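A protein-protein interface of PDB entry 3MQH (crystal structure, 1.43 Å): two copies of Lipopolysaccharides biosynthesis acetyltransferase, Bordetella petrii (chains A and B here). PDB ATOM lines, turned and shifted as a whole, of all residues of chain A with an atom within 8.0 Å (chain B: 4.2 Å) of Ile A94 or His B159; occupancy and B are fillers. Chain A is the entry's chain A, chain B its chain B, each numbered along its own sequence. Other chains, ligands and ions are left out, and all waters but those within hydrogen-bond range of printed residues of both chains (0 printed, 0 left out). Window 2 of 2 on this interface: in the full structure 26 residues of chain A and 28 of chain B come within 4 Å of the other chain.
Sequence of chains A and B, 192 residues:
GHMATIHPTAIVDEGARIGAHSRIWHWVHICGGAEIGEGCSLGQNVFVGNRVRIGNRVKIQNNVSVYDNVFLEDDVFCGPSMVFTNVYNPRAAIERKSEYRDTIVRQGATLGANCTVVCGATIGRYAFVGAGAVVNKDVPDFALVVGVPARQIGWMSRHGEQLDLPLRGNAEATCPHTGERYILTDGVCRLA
No position is printed for both chains.
Of the 11 printed residues of chain A, 4 touch a printed residue of chain B.
Hydrophobic or aromatic side chains of chain A that line the printed part of chain B: Ile A94.
Hydrophobic or aromatic side chains of chain B that line the printed part of chain A: His B159.
Among the printed residues, 7 pairs touch across the chains.
Among the printed residues, merely in contact across the chains: Arg A91 with His B159 (3.7 Å), Arg A91 with Gly B160 (3.9 Å) and Ile A94 with His B159 (3.7 Å).
O of Asn A89 lies within hydrogen-bond range of NH1 of Arg A96 (2.9 Å).
The guanidinium group of Arg A96 lies within salt-bridge range of the side-chain carboxylate of Glu A99 (3.0 Å).
The side-chain hydroxyl (OG) of Ser B157 is in hydrogen-bond range of the backbone NH (N) of Gly B160, 3.2 Å away.
The side-chain hydroxyl of Ser B157 is in hydrogen-bond range of the backbone carbonyl oxygen of Glu B161 (3.1 Å).
The side-chain hydroxyl (OG) of Ser B157 sits close to the backbone NH (N) of His B159, 3.3 Å away.
O of Ser B157 is in hydrogen-bond range of NH2 of Arg A91.
The side-chain amide nitrogen (ND2) of Asn A89 sits at hydrogen-bond distance from the backbone carbonyl oxygen (O) of Gly B160 (2.9 Å).
O of Arg B158 is in hydrogen-bond range of NE of Arg A91 (2.9 Å).
The guanidinium group (NH2) of Arg A96 lies within hydrogen-bond range of the backbone carbonyl oxygen (O) of His B159.
Printed residues of chain B within 4 Å of Asn A89: Gly B160.
Of the printed residues of chain B, Arg A91 touches Ser B157 (2.9 Å), Arg B158 (2.9 Å), His B159 (3.7 Å) and Gly B160 (3.9 Å).
Ile A94 touches just one residue of chain B: His B159.
Printed residues of chain B within 4 Å of Arg A96: His B159 (2.8 Å).
Of the printed residues of chain A, Arg B158 touches Arg A91.
His B159 touches just these residues of chain A: Arg A91 (3.7 Å), Ile A94 (3.7 Å) and Arg A96 (2.8 Å).
Printed residues of chain A within 4 Å of Gly B160: Asn A89 and Arg A91.
The nearest printed residue of chain B that does not touch Ile A94 is Arg B158 (4.4 Å).
The nearest residue of chain A that does not touch His B159 is Asn A89 (4.3 Å).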
ATOM      1  N   VAL A  87      -1.270   1.453  -2.485  1.00  0.00           N
ATOM      2  CA  VAL A  87      -1.594   2.855  -2.307  1.00  0.00           C
ATOM      3  C   VAL A  87      -2.344   3.335  -3.537  1.00  0.00           C
ATOM      4  O   VAL A  87      -1.951   3.122  -4.677  1.00  0.00           O
ATOM      5  CB  VAL A  87      -0.319   3.708  -2.079  1.00  0.00           C
ATOM      6  CG1 VAL A  87      -0.625   5.197  -2.118  1.00  0.00           C
ATOM      7  CG2 VAL A  87       0.320   3.319  -0.706  1.00  0.00           C
ATOM      8  N   ASN A  89      -3.195   6.511  -4.491  1.00  0.00           N
ATOM      9  CA  ASN A  89      -2.767   7.771  -5.127  1.00  0.00           C
ATOM     10  C   ASN A  89      -1.345   8.094  -4.711  1.00  0.00           C
ATOM     11  O   ASN A  89      -1.108   9.079  -3.988  1.00  0.00           O
ATOM     12  CB  ASN A  89      -3.686   8.915  -4.688  1.00  0.00           C
ATOM     13  CG  ASN A  89      -3.778   9.097  -3.181  1.00  0.00           C
ATOM     14  OD1 ASN A  89      -3.625   8.150  -2.396  1.00  0.00           O
ATOM     15  ND2 ASN A  89      -4.051  10.355  -2.749  1.00  0.00           N
ATOM     16  N   PRO A  90      -0.366   7.260  -5.096  1.00  0.00           N
ATOM     17  CA  PRO A  90       0.983   7.458  -4.574  1.00  0.00           C
ATOM     18  C   PRO A  90       1.642   8.752  -5.106  1.00  0.00           C
ATOM     19  O   PRO A  90       1.448   9.163  -6.257  1.00  0.00           O
ATOM     20  CB  PRO A  90       1.749   6.204  -5.028  1.00  0.00           C
ATOM     21  CG  PRO A  90       0.997   5.733  -6.273  1.00  0.00           C
ATOM     22  CD  PRO A  90      -0.467   6.093  -6.000  1.00  0.00           C
ATOM     23  N   ARG A  91       2.420   9.362  -4.209  1.00  0.00           N
ATOM     24  CA  ARG A  91       3.310  10.495  -4.505  1.00  0.00           C
ATOM     25  C   ARG A  91       4.613  10.213  -3.759  1.00  0.00           C
ATOM     26  O   ARG A  91       4.576  10.003  -2.547  1.00  0.00           O
ATOM     27  CB  ARG A  91       2.690  11.815  -3.973  1.00  0.00           C
ATOM     28  CG  ARG A  91       1.495  12.321  -4.810  1.00  0.00           C
ATOM     29  CD  ARG A  91       1.986  12.701  -6.195  1.00  0.00           C
ATOM     30  NE  ARG A  91       1.052  13.638  -6.799  1.00  0.00           N
ATOM     31  CZ  ARG A  91       0.879  13.784  -8.115  1.00  0.00           C
ATOM     32  NH1 ARG A  91       1.526  13.030  -9.001  1.00  0.00           N
ATOM     33  NH2 ARG A  91       0.019  14.674  -8.610  1.00  0.00           N
ATOM     34  N   ALA A  92       5.748  10.212  -4.466  1.00  0.00           N
ATOM     35  CA  ALA A  92       7.020   9.866  -3.838  1.00  0.00           C
ATOM     36  C   ALA A  92       7.316  10.784  -2.630  1.00  0.00           C
ATOM     37  O   ALA A  92       7.955  10.339  -1.662  1.00  0.00           O
ATOM     38  CB  ALA A  92       8.155   9.885  -4.885  1.00  0.00           C
ATOM     39  N   ALA A  93       6.859  12.024  -2.690  1.00  0.00           N
ATOM     40  CA  ALA A  93       7.175  12.975  -1.612  1.00  0.00           C
ATOM     41  C   ALA A  93       6.373  12.715  -0.352  1.00  0.00           C
ATOM     42  O   ALA A  93       6.730  13.249   0.713  1.00  0.00           O
ATOM     43  CB  ALA A  93       6.942  14.405  -2.091  1.00  0.00           C
ATOM     44  N   ILE A  94       5.276  11.960  -0.433  1.00  0.00           N
ATOM     45  CA  ILE A  94       4.362  11.804   0.700  1.00  0.00           C
ATOM     46  C   ILE A  94       4.320  10.313   1.065  1.00  0.00           C
ATOM     47  O   ILE A  94       3.690   9.524   0.357  1.00  0.00           O
ATOM     48  CB  ILE A  94       2.953  12.345   0.414  1.00  0.00           C
ATOM     49  CG1 ILE A  94       2.992  13.815  -0.011  1.00  0.00           C
ATOM     50  CG2 ILE A  94       2.046  12.105   1.644  1.00  0.00           C
ATOM     51  CD1 ILE A  94       1.672  14.262  -0.625  1.00  0.00           C
ATOM     52  N   GLU A  95       4.989   9.878   2.122  1.00  0.00           N
ATOM     53  CA  GLU A  95       4.962   8.467   2.462  1.00  0.00           C
ATOM     54  C   GLU A  95       3.534   8.102   2.869  1.00  0.00           C
ATOM     55  O   GLU A  95       2.919   8.734   3.724  1.00  0.00           O
ATOM     56  CB  GLU A  95       5.965   8.210   3.594  1.00  0.00           C
ATOM     57  CG  GLU A  95       6.011   6.780   4.134  1.00  0.00           C
ATOM     58  CD  GLU A  95       7.135   6.624   5.150  1.00  0.00           C
ATOM     59  OE1 GLU A  95       8.307   6.967   4.848  1.00  0.00           O
ATOM     60  OE2 GLU A  95       6.816   6.161   6.265  1.00  0.00           O
ATOM     61  N   ARG A  96       2.998   7.062   2.218  1.00  0.00           N
ATOM     62  CA  ARG A  96       1.615   6.649   2.411  1.00  0.00           C
ATOM     63  C   ARG A  96       1.480   5.256   2.998  1.00  0.00           C
ATOM     64  O   ARG A  96       0.415   4.627   2.842  1.00  0.00           O
ATOM     65  CB  ARG A  96       0.756   6.877   1.153  1.00  0.00           C
ATOM     66  CG  ARG A  96       0.315   8.359   1.020  1.00  0.00           C
ATOM     67  CD  ARG A  96      -0.614   8.670  -0.167  1.00  0.00           C
ATOM     68  NE  ARG A  96      -1.225   9.993   0.066  1.00  0.00           N
ATOM     69  CZ  ARG A  96      -1.101  11.047  -0.733  1.00  0.00           C
ATOM     70  NH1 ARG A  96      -0.487  10.978  -1.914  1.00  0.00           N
ATOM     71  NH2 ARG A  96      -1.647  12.215  -0.365  1.00  0.00           N
ATOM     72  N   LYS A  97       2.537   4.804   3.667  1.00  0.00           N
ATOM     73  CA  LYS A  97       2.553   3.477   4.288  1.00  0.00           C
ATOM     74  C   LYS A  97       1.429   3.335   5.310  1.00  0.00           C
ATOM     75  O   LYS A  97       0.987   2.213   5.532  1.00  0.00           O
ATOM     76  CB  LYS A  97       3.925   3.150   4.906  1.00  0.00           C
ATOM     77  CG  LYS A  97       5.074   3.032   3.884  1.00  0.00           C
ATOM     78  CD  LYS A  97       6.444   2.826   4.555  1.00  0.00           C
ATOM     79  CE  LYS A  97       7.585   3.247   3.627  1.00  0.00           C
ATOM     80  NZ  LYS A  97       8.911   3.123   4.316  1.00  0.00           N
ATOM     81  N   GLU A  99      -1.620   4.529   4.824  1.00  0.00           N
ATOM     82  CA  GLU A  99      -2.854   4.700   4.044  1.00  0.00           C
ATOM     83  C   GLU A  99      -3.135   3.508   3.117  1.00  0.00           C
ATOM     84  O   GLU A  99      -3.973   3.603   2.215  1.00  0.00           O
ATOM     85  CB  GLU A  99      -2.822   5.988   3.193  1.00  0.00           C
ATOM     86  CG  GLU A  99      -2.659   7.220   4.091  1.00  0.00           C
ATOM     87  CD  GLU A  99      -2.568   8.520   3.339  1.00  0.00           C
ATOM     88  OE1 GLU A  99      -2.845   8.556   2.125  1.00  0.00           O
ATOM     89  OE2 GLU A  99      -2.249   9.545   3.998  1.00  0.00           O
ATOM     90  N   SER B 157      -3.770  17.532  -7.892  1.00  0.00           N
ATOM     91  CA  SER B 157      -2.900  18.373  -7.073  1.00  0.00           C
ATOM     92  C   SER B 157      -1.575  17.652  -6.739  1.00  0.00           C
ATOM     93  O   SER B 157      -1.402  16.449  -6.870  1.00  0.00           O
ATOM     94  CB  SER B 157      -3.641  18.629  -5.764  1.00  0.00           C
ATOM     95  OG  SER B 157      -3.727  17.407  -5.035  1.00  0.00           O
ATOM     96  N   ARG B 158      -0.587  18.419  -6.284  1.00  0.00           N
ATOM     97  CA  ARG B 158       0.636  17.804  -5.740  1.00  0.00           C
ATOM     98  C   ARG B 158       0.334  16.724  -4.729  1.00  0.00           C
ATOM     99  O   ARG B 158       0.989  15.670  -4.724  1.00  0.00           O
ATOM    100  CB  ARG B 158       1.590  18.802  -5.082  1.00  0.00           C
ATOM    101  CG  ARG B 158       2.099  19.880  -6.031  1.00  0.00           C
ATOM    102  CD  ARG B 158       3.362  20.565  -5.494  1.00  0.00           C
ATOM    103  NE  ARG B 158       3.055  21.553  -4.468  1.00  0.00           N
ATOM    104  CZ  ARG B 158       3.914  22.488  -4.062  1.00  0.00           C
ATOM    105  NH1 ARG B 158       5.126  22.540  -4.596  1.00  0.00           N
ATOM    106  NH2 ARG B 158       3.578  23.375  -3.132  1.00  0.00           N
ATOM    107  N   HIS B 159      -0.640  16.960  -3.854  1.00  0.00           N
ATOM    108  CA  HIS B 159      -1.004  16.023  -2.803  1.00  0.00           C
ATOM    109  C   HIS B 159      -1.459  14.716  -3.424  1.00  0.00           C
ATOM    110  O   HIS B 159      -1.288  13.665  -2.782  1.00  0.00           O
ATOM    111  CB  HIS B 159      -2.179  16.646  -2.053  1.00  0.00           C
ATOM    112  CG  HIS B 159      -2.716  15.809  -0.937  1.00  0.00           C
ATOM    113  ND1 HIS B 159      -2.155  15.764   0.323  1.00  0.00           N
ATOM    114  CD2 HIS B 159      -3.787  14.984  -0.905  1.00  0.00           C
ATOM    115  CE1 HIS B 159      -2.880  14.964   1.095  1.00  0.00           C
ATOM    116  NE2 HIS B 159      -3.869  14.463   0.365  1.00  0.00           N
ATOM    117  N   GLY B 160      -2.051  14.766  -4.620  1.00  0.00           N
ATOM    118  CA  GLY B 160      -2.504  13.539  -5.311  1.00  0.00           C
ATOM    119  C   GLY B 160      -3.989  13.259  -5.182  1.00  0.00           C
ATOM    120  O   GLY B 160      -4.415  12.116  -5.072  1.00  0.00           O
ATOM    121  N   GLU B 161      -4.795  14.316  -5.213  1.00  0.00           N
ATOM    122  CA  GLU B 161      -6.237  14.144  -5.364  1.00  0.00           C
ATOM    123  C   GLU B 161      -6.705  15.128  -6.419  1.00  0.00           C
ATOM    124  O   GLU B 161      -6.087  16.167  -6.690  1.00  0.00           O
ATOM    125  CB  GLU B 161      -7.028  14.421  -4.083  1.00  0.00           C
ATOM    126  CG  GLU B 161      -6.778  13.400  -2.977  1.00  0.00           C
ATOM    127  CD  GLU B 161      -7.431  13.709  -1.676  1.00  0.00           C
ATOM    128  OE1 GLU B 161      -8.395  14.500  -1.618  1.00  0.00           O
ATOM    129  OE2 GLU B 161      -6.959  13.117  -0.678  1.00  0.00           O
ATOM    130  N   HIS B 177      -6.057  20.360   1.099  1.00  0.00           N
ATOM    131  CA  HIS B 177      -5.121  19.862   2.088  1.00  0.00           C
ATOM    132  C   HIS B 177      -4.060  20.881   2.465  1.00  0.00           C
ATOM    133  O   HIS B 177      -3.613  20.915   3.622  1.00  0.00           O
ATOM    134  CB  HIS B 177      -4.455  18.609   1.528  1.00  0.00           C
ATOM    135  CG  HIS B 177      -5.475  17.541   1.258  1.00  0.00           C
ATOM    136  ND1 HIS B 177      -6.003  16.770   2.274  1.00  0.00           N
ATOM    137  CD2 HIS B 177      -6.106  17.154   0.117  1.00  0.00           C
ATOM    138  CE1 HIS B 177      -6.897  15.939   1.767  1.00  0.00           C
ATOM    139  NE2 HIS B 177      -6.998  16.166   0.470  1.00  0.00           N
